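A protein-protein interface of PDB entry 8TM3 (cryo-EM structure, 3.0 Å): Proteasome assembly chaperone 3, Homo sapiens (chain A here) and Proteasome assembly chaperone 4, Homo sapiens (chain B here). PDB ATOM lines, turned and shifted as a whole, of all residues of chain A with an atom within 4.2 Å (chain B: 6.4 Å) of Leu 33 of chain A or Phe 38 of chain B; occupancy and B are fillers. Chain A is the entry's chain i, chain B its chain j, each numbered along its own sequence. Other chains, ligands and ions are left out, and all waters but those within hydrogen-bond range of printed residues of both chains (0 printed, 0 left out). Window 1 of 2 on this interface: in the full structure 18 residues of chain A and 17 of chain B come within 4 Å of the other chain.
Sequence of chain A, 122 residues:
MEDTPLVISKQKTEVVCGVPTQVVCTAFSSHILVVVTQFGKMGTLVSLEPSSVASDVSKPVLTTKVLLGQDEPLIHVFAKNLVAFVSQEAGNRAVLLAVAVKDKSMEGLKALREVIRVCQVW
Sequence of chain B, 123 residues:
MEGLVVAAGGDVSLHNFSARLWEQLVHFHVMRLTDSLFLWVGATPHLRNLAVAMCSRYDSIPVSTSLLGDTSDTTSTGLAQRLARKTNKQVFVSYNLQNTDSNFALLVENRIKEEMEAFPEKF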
ATOM      1  N   VAL A  24      12.147  -2.646  12.595  1.00  0.00           N
ATOM      2  CA  VAL A  24      11.542  -3.941  12.885  1.00  0.00           C
ATOM      3  C   VAL A  24      12.362  -4.606  13.979  1.00  0.00           C
ATOM      4  O   VAL A  24      13.597  -4.535  13.970  1.00  0.00           O
ATOM      5  CB  VAL A  24      11.477  -4.837  11.636  1.00  0.00           C
ATOM      6  CG1 VAL A  24      10.776  -6.144  11.965  1.00  0.00           C
ATOM      7  CG2 VAL A  24      10.776  -4.123  10.492  1.00  0.00           C
ATOM      8  N   CYS A  25      11.678  -5.251  14.921  1.00  0.00           N
ATOM      9  CA  CYS A  25      12.325  -5.921  16.046  1.00  0.00           C
ATOM     10  C   CYS A  25      11.678  -7.290  16.222  1.00  0.00           C
ATOM     11  O   CYS A  25      10.587  -7.399  16.788  1.00  0.00           O
ATOM     12  CB  CYS A  25      12.214  -5.084  17.314  1.00  0.00           C
ATOM     13  SG  CYS A  25      12.722  -3.372  17.082  1.00  0.00           S
ATOM     14  N   THR A  26      12.352  -8.327  15.737  1.00  0.00           N
ATOM     15  CA  THR A  26      11.892  -9.703  15.855  1.00  0.00           C
ATOM     16  C   THR A  26      12.672 -10.386  16.969  1.00  0.00           C
ATOM     17  O   THR A  26      13.906 -10.362  16.973  1.00  0.00           O
ATOM     18  CB  THR A  26      12.075 -10.457  14.537  1.00  0.00           C
ATOM     19  OG1 THR A  26      13.382 -11.040  14.495  1.00  0.00           O
ATOM     20  CG2 THR A  26      11.902  -9.519  13.351  1.00  0.00           C
ATOM     21  N   HIS A  31      19.277 -14.464  19.247  1.00  0.00           N
ATOM     22  CA  HIS A  31      19.627 -13.145  18.730  1.00  0.00           C
ATOM     23  C   HIS A  31      18.356 -12.410  18.328  1.00  0.00           C
ATOM     24  O   HIS A  31      17.674 -12.819  17.384  1.00  0.00           O
ATOM     25  CB  HIS A  31      20.576 -13.254  17.537  1.00  0.00           C
ATOM     26  CG  HIS A  31      21.859 -13.959  17.842  1.00  0.00           C
ATOM     27  ND1 HIS A  31      22.051 -15.300  17.586  1.00  0.00           N
ATOM     28  CD2 HIS A  31      23.020 -13.508  18.374  1.00  0.00           C
ATOM     29  CE1 HIS A  31      23.272 -15.645  17.952  1.00  0.00           C
ATOM     30  NE2 HIS A  31      23.880 -14.577  18.433  1.00  0.00           N
ATOM     31  N   ILE A  32      18.048 -11.322  19.030  1.00  0.00           N
ATOM     32  CA  ILE A  32      16.958 -10.450  18.610  1.00  0.00           C
ATOM     33  C   ILE A  32      17.421  -9.631  17.415  1.00  0.00           C
ATOM     34  O   ILE A  32      18.502  -9.030  17.434  1.00  0.00           O
ATOM     35  CB  ILE A  32      16.511  -9.549  19.770  1.00  0.00           C
ATOM     36  CG1 ILE A  32      15.935 -10.406  20.899  1.00  0.00           C
ATOM     37  CG2 ILE A  32      15.482  -8.528  19.285  1.00  0.00           C
ATOM     38  CD1 ILE A  32      15.457  -9.618  22.100  1.00  0.00           C
ATOM     39  N   LEU A  33      16.605  -9.605  16.364  1.00  0.00           N
ATOM     40  CA  LEU A  33      16.955  -8.938  15.115  1.00  0.00           C
ATOM     41  C   LEU A  33      16.313  -7.555  15.099  1.00  0.00           C
ATOM     42  O   LEU A  33      15.085  -7.433  15.141  1.00  0.00           O
ATOM     43  CB  LEU A  33      16.500  -9.768  13.917  1.00  0.00           C
ATOM     44  CG  LEU A  33      16.965  -9.326  12.525  1.00  0.00           C
ATOM     45  CD1 LEU A  33      18.356  -8.708  12.552  1.00  0.00           C
ATOM     46  CD2 LEU A  33      16.925 -10.502  11.563  1.00  0.00           C
ATOM     47  N   VAL A  34      17.145  -6.522  15.035  1.00  0.00           N
ATOM     48  CA  VAL A  34      16.691  -5.137  14.978  1.00  0.00           C
ATOM     49  C   VAL A  34      16.957  -4.628  13.568  1.00  0.00           C
ATOM     50  O   VAL A  34      18.103  -4.346  13.206  1.00  0.00           O
ATOM     51  CB  VAL A  34      17.401  -4.270  16.026  1.00  0.00           C
ATOM     52  CG1 VAL A  34      16.947  -2.823  15.914  1.00  0.00           C
ATOM     53  CG2 VAL A  34      17.146  -4.814  17.421  1.00  0.00           C
ATOM     54  N   VAL A  35      15.900  -4.495  12.770  1.00  0.00           N
ATOM     55  CA  VAL A  35      16.045  -4.105  11.373  1.00  0.00           C
ATOM     56  C   VAL A  35      15.653  -2.645  11.205  1.00  0.00           C
ATOM     57  O   VAL A  35      14.470  -2.321  11.050  1.00  0.00           O
ATOM     58  CB  VAL A  35      15.204  -5.006  10.450  1.00  0.00           C
ATOM     59  CG1 VAL A  35      15.604  -4.803   8.997  1.00  0.00           C
ATOM     60  CG2 VAL A  35      15.347  -6.465  10.853  1.00  0.00           C
ATOM     61  N   LEU A  96      21.423  -8.563  17.002  1.00  0.00           N
ATOM     62  CA  LEU A  96      21.873  -8.204  15.666  1.00  0.00           C
ATOM     63  C   LEU A  96      21.106  -6.983  15.173  1.00  0.00           C
ATOM     64  O   LEU A  96      19.938  -6.785  15.515  1.00  0.00           O
ATOM     65  CB  LEU A  96      21.675  -9.364  14.691  1.00  0.00           C
ATOM     66  CG  LEU A  96      22.887 -10.270  14.474  1.00  0.00           C
ATOM     67  CD1 LEU A  96      23.326 -10.900  15.787  1.00  0.00           C
ATOM     68  CD2 LEU A  96      22.572 -11.337  13.438  1.00  0.00           C
ATOM     69  N   HIS B  29       9.378 -17.018   9.352  1.00  0.00           N
ATOM     70  CA  HIS B  29       9.322 -15.566   9.438  1.00  0.00           C
ATOM     71  C   HIS B  29       9.665 -14.981   8.077  1.00  0.00           C
ATOM     72  O   HIS B  29      10.484 -15.542   7.345  1.00  0.00           O
ATOM     73  CB  HIS B  29      10.286 -15.032  10.506  1.00  0.00           C
ATOM     74  CG  HIS B  29       9.967 -13.646  10.971  1.00  0.00           C
ATOM     75  ND1 HIS B  29       9.974 -12.555  10.128  1.00  0.00           N
ATOM     76  CD2 HIS B  29       9.625 -13.173  12.193  1.00  0.00           C
ATOM     77  CE1 HIS B  29       9.655 -11.471  10.811  1.00  0.00           C
ATOM     78  NE2 HIS B  29       9.438 -11.818  12.066  1.00  0.00           N
ATOM     79  N   VAL B  30       9.035 -13.858   7.741  1.00  0.00           N
ATOM     80  CA  VAL B  30       9.248 -13.186   6.465  1.00  0.00           C
ATOM     81  C   VAL B  30       9.401 -11.694   6.721  1.00  0.00           C
ATOM     82  O   VAL B  30       8.673 -11.122   7.539  1.00  0.00           O
ATOM     83  CB  VAL B  30       8.092 -13.450   5.482  1.00  0.00           C
ATOM     84  CG1 VAL B  30       8.066 -12.395   4.384  1.00  0.00           C
ATOM     85  CG2 VAL B  30       8.217 -14.842   4.889  1.00  0.00           C
ATOM     86  N   MET B  31      10.353 -11.071   6.029  1.00  0.00           N
ATOM     87  CA  MET B  31      10.544  -9.623   6.057  1.00  0.00           C
ATOM     88  C   MET B  31      10.760  -9.166   4.621  1.00  0.00           C
ATOM     89  O   MET B  31      11.856  -9.320   4.076  1.00  0.00           O
ATOM     90  CB  MET B  31      11.726  -9.233   6.945  1.00  0.00           C
ATOM     91  N   ARG B  32       9.716  -8.600   4.013  1.00  0.00           N
ATOM     92  CA  ARG B  32       9.758  -8.331   2.579  1.00  0.00           C
ATOM     93  C   ARG B  32      10.740  -7.216   2.239  1.00  0.00           C
ATOM     94  O   ARG B  32      11.499  -7.328   1.269  1.00  0.00           O
ATOM     95  CB  ARG B  32       8.362  -7.972   2.075  1.00  0.00           C
ATOM     96  CG  ARG B  32       7.376  -9.129   2.114  1.00  0.00           C
ATOM     97  CD  ARG B  32       7.610 -10.121   0.983  1.00  0.00           C
ATOM     98  NE  ARG B  32       7.753  -9.470  -0.314  1.00  0.00           N
ATOM     99  CZ  ARG B  32       6.761  -8.895  -0.979  1.00  0.00           C
ATOM    100  NH1 ARG B  32       5.528  -8.868  -0.497  1.00  0.00           N
ATOM    101  NH2 ARG B  32       7.010  -8.333  -2.158  1.00  0.00           N
ATOM    102  N   LEU B  33      10.743  -6.136   3.017  1.00  0.00           N
ATOM    103  CA  LEU B  33      11.495  -4.947   2.641  1.00  0.00           C
ATOM    104  C   LEU B  33      11.033  -4.488   1.262  1.00  0.00           C
ATOM    105  O   LEU B  33       9.835  -4.269   1.053  1.00  0.00           O
ATOM    106  CB  LEU B  33      12.998  -5.233   2.659  1.00  0.00           C
ATOM    107  N   SER B  36      14.899  -7.369  -0.649  1.00  0.00           N
ATOM    108  CA  SER B  36      15.762  -8.145   0.239  1.00  0.00           C
ATOM    109  C   SER B  36      14.897  -8.956   1.204  1.00  0.00           C
ATOM    110  O   SER B  36      14.796  -8.678   2.401  1.00  0.00           O
ATOM    111  CB  SER B  36      16.718  -7.223   0.982  1.00  0.00           C
ATOM    112  OG  SER B  36      17.845  -7.935   1.458  1.00  0.00           O
ATOM    113  N   LEU B  37      14.261  -9.984   0.652  1.00  0.00           N
ATOM    114  CA  LEU B  37      13.449 -10.876   1.467  1.00  0.00           C
ATOM    115  C   LEU B  37      14.306 -11.541   2.536  1.00  0.00           C
ATOM    116  O   LEU B  37      15.453 -11.922   2.290  1.00  0.00           O
ATOM    117  CB  LEU B  37      12.789 -11.936   0.585  1.00  0.00           C
ATOM    118  CG  LEU B  37      11.981 -13.015   1.308  1.00  0.00           C
ATOM    119  CD1 LEU B  37      10.728 -12.420   1.923  1.00  0.00           C
ATOM    120  CD2 LEU B  37      11.628 -14.140   0.348  1.00  0.00           C
ATOM    121  N   PHE B  38      13.747 -11.667   3.735  1.00  0.00           N
ATOM    122  CA  PHE B  38      14.380 -12.380   4.835  1.00  0.00           C
ATOM    123  C   PHE B  38      13.503 -13.560   5.220  1.00  0.00           C
ATOM    124  O   PHE B  38      12.294 -13.400   5.416  1.00  0.00           O
ATOM    125  CB  PHE B  38      14.594 -11.462   6.040  1.00  0.00           C
ATOM    126  CG  PHE B  38      14.925 -12.196   7.310  1.00  0.00           C
ATOM    127  CD1 PHE B  38      16.235 -12.516   7.619  1.00  0.00           C
ATOM    128  CD2 PHE B  38      13.927 -12.563   8.195  1.00  0.00           C
ATOM    129  CE1 PHE B  38      16.542 -13.190   8.784  1.00  0.00           C
ATOM    130  CE2 PHE B  38      14.230 -13.238   9.361  1.00  0.00           C
ATOM    131  CZ  PHE B  38      15.539 -13.551   9.655  1.00  0.00           C
ATOM    132  N   LEU B  39      14.108 -14.739   5.326  1.00  0.00           N
ATOM    133  CA  LEU B  39      13.391 -15.957   5.681  1.00  0.00           C
ATOM    134  C   LEU B  39      14.095 -16.623   6.852  1.00  0.00           C
ATOM    135  O   LEU B  39      15.321 -16.766   6.842  1.00  0.00           O
ATOM    136  CB  LEU B  39      13.314 -16.919   4.492  1.00  0.00           C
ATOM    137  CG  LEU B  39      12.473 -18.182   4.701  1.00  0.00           C
ATOM    138  CD1 LEU B  39      11.012 -17.830   4.914  1.00  0.00           C
ATOM    139  CD2 LEU B  39      12.627 -19.129   3.521  1.00  0.00           C
ATOM    140  N   TRP B  40      13.321 -17.022   7.856  1.00  0.00           N
ATOM    141  CA  TRP B  40      13.832 -17.751   9.006  1.00  0.00           C
ATOM    142  C   TRP B  40      13.111 -19.085   9.116  1.00  0.00           C
ATOM    143  O   TRP B  40      11.918 -19.182   8.811  1.00  0.00           O
ATOM    144  CB  TRP B  40      13.649 -16.957  10.301  1.00  0.00           C
ATOM    145  CG  TRP B  40      13.842 -17.788  11.527  1.00  0.00           C
ATOM    146  CD1 TRP B  40      15.027 -18.210  12.054  1.00  0.00           C
ATOM    147  CD2 TRP B  40      12.816 -18.315  12.376  1.00  0.00           C
ATOM    148  NE1 TRP B  40      14.803 -18.960  13.182  1.00  0.00           N
ATOM    149  CE2 TRP B  40      13.453 -19.040  13.401  1.00  0.00           C
ATOM    150  CE3 TRP B  40      11.420 -18.239  12.371  1.00  0.00           C
ATOM    151  CZ2 TRP B  40      12.743 -19.685  14.410  1.00  0.00           C
ATOM    152  CZ3 TRP B  40      10.718 -18.880  13.373  1.00  0.00           C
ATOM    153  CH2 TRP B  40      11.380 -19.592  14.379  1.00  0.00           C
ATOM    154  N   LEU B  47      18.546 -17.846  16.145  1.00  0.00           N
ATOM    155  CA  LEU B  47      19.258 -17.428  14.939  1.00  0.00           C
ATOM    156  C   LEU B  47      20.616 -18.125  14.898  1.00  0.00           C
ATOM    157  O   LEU B  47      21.672 -17.529  15.110  1.00  0.00           O
ATOM    158  CB  LEU B  47      19.408 -15.909  14.911  1.00  0.00           C
ATOM    159  CG  LEU B  47      18.244 -15.048  14.409  1.00  0.00           C
ATOM    160  CD1 LEU B  47      18.687 -13.599  14.272  1.00  0.00           C
ATOM    161  CD2 LEU B  47      17.693 -15.541  13.082  1.00  0.00           C
ATOM    162  N   LEU B  50      22.819 -18.169   9.218  1.00  0.00           N
ATOM    163  CA  LEU B  50      22.273 -17.127   8.358  1.00  0.00           C
ATOM    164  C   LEU B  50      23.175 -16.972   7.145  1.00  0.00           C
ATOM    165  O   LEU B  50      24.399 -16.885   7.290  1.00  0.00           O
ATOM    166  CB  LEU B  50      22.155 -15.797   9.108  1.00  0.00           C
ATOM    167  CG  LEU B  50      21.611 -14.611   8.308  1.00  0.00           C
ATOM    168  CD1 LEU B  50      20.123 -14.770   8.050  1.00  0.00           C
ATOM    169  CD2 LEU B  50      21.891 -13.308   9.035  1.00  0.00           C
ATOM    170  N   GLN B  90      17.950 -10.196  -2.815  1.00  0.00           N
ATOM    171  CA  GLN B  90      18.533 -10.909  -1.687  1.00  0.00           C
ATOM    172  C   GLN B  90      17.510 -11.815  -1.016  1.00  0.00           C
ATOM    173  O   GLN B  90      16.305 -11.551  -1.045  1.00  0.00           O
ATOM    174  CB  GLN B  90      19.095  -9.922  -0.661  1.00  0.00           C
ATOM    175  CG  GLN B  90      19.554  -8.591  -1.240  1.00  0.00           C
ATOM    176  CD  GLN B  90      20.210  -7.701  -0.206  1.00  0.00           C
ATOM    177  OE1 GLN B  90      19.574  -6.813   0.360  1.00  0.00           O
ATOM    178  NE2 GLN B  90      21.491  -7.936   0.049  1.00  0.00           N
ATOM    179  N   VAL B  91      18.007 -12.892  -0.414  1.00  0.00           N
ATOM    180  CA  VAL B  91      17.205 -13.805   0.391  1.00  0.00           C
ATOM    181  C   VAL B  91      18.052 -14.192   1.595  1.00  0.00           C
ATOM    182  O   VAL B  91      19.045 -14.914   1.452  1.00  0.00           O
ATOM    183  CB  VAL B  91      16.768 -15.048  -0.394  1.00  0.00           C
ATOM    184  CG1 VAL B  91      15.777 -15.864   0.422  1.00  0.00           C
ATOM    185  CG2 VAL B  91      16.166 -14.647  -1.731  1.00  0.00           C
ATOM    186  N   PHE B  92      17.661 -13.719   2.779  1.00  0.00           N
ATOM    187  CA  PHE B  92      18.407 -13.988   4.008  1.00  0.00           C
ATOM    188  C   PHE B  92      17.805 -15.218   4.681  1.00  0.00           C
ATOM    189  O   PHE B  92      16.925 -15.135   5.540  1.00  0.00           O
ATOM    190  CB  PHE B  92      18.376 -12.775   4.928  1.00  0.00           C
ATOM    191  CG  PHE B  92      19.240 -11.638   4.466  1.00  0.00           C
ATOM    192  CD1 PHE B  92      18.899 -10.903   3.346  1.00  0.00           C
ATOM    193  CD2 PHE B  92      20.385 -11.296   5.163  1.00  0.00           C
ATOM    194  CE1 PHE B  92      19.689  -9.856   2.923  1.00  0.00           C
ATOM    195  CE2 PHE B  92      21.178 -10.247   4.744  1.00  0.00           C
ATOM    196  CZ  PHE B  92      20.828  -9.526   3.624  1.00  0.00           C
ATOM    197  N   VAL B  93      18.295 -16.382   4.276  1.00  0.00           N
ATOM    198  CA  VAL B  93      17.840 -17.643   4.848  1.00  0.00           C
ATOM    199  C   VAL B  93      18.566 -17.883   6.162  1.00  0.00           C
ATOM    200  O   VAL B  93      19.770 -17.629   6.280  1.00  0.00           O
ATOM    201  CB  VAL B  93      18.073 -18.799   3.862  1.00  0.00           C
ATOM    202  CG1 VAL B  93      17.904 -20.135   4.567  1.00  0.00           C
ATOM    203  CG2 VAL B  93      17.130 -18.683   2.680  1.00  0.00           C
ATOM    204  N   SER B  94      17.835 -18.378   7.158  1.00  0.00           N
ATOM    205  CA  SER B  94      18.368 -18.615   8.495  1.00  0.00           C
ATOM    206  C   SER B  94      17.946 -19.986   9.008  1.00  0.00           C
ATOM    207  O   SER B  94      17.430 -20.131  10.117  1.00  0.00           O
ATOM    208  CB  SER B  94      17.918 -17.527   9.461  1.00  0.00           C
ATOM    209  OG  SER B  94      18.528 -17.702  10.727  1.00  0.00           O
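Of the 9 printed residues of chain A, 3 touch a printed residue of chain B.
Hydrophobic or aromatic side chains of chain A within 4 Å of the printed part of chain B: His 31 and Leu 33.
A ring nitrogen (ND1) of His 31 of chain A lies within hydrogen-bond range of the backbone carbonyl oxygen of Leu 47 of chain B (3.4 Å).
Leu 33 of chain A touches one residue of chain B.
Phe 38 of chain B touches one residue of chain A.
Printed residues of chain B within 4 Å of His 31 of chain A: Leu 47 (3.4 Å).
Of the printed residues of chain A, Leu 47 of chain B touches His 31 (3.4 Å).
Val 24 of chain A touches none of the printed residues of chain B.
The nearest residue of chain B that does not touch Leu 33 of chain A is Leu 47 of chain B (4.4 Å).
The nearest printed residue of chain A that does not touch Phe 38 of chain B is Thr 26 of chain A (5.6 Å).
The nearest printed residue of chain B that does not touch His 31 of chain A is Trp 40 of chain B (8.0 Å).
The backbone NH (N) of Trp 40 of chain B is in hydrogen-bond range of the backbone carbonyl oxygen (O) of His 29 of chain B, 3.2 Å away.
The backbone NH (N) of Phe 38 of chain B sits at hydrogen-bond distance from the backbone carbonyl oxygen (O) of Met 31 of chain B (3.0 Å).
O of Thr 26 of chain A lies within hydrogen-bond range of N of Leu 33 of chain A (2.9 Å).
CG2 of Thr 26 of chain A touches NE2 of His 29 of chain B, at 3.6 Å.
Leu 33 of chain A touches Phe 38 of chain B (CD2 to CZ, 3.9 Å).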
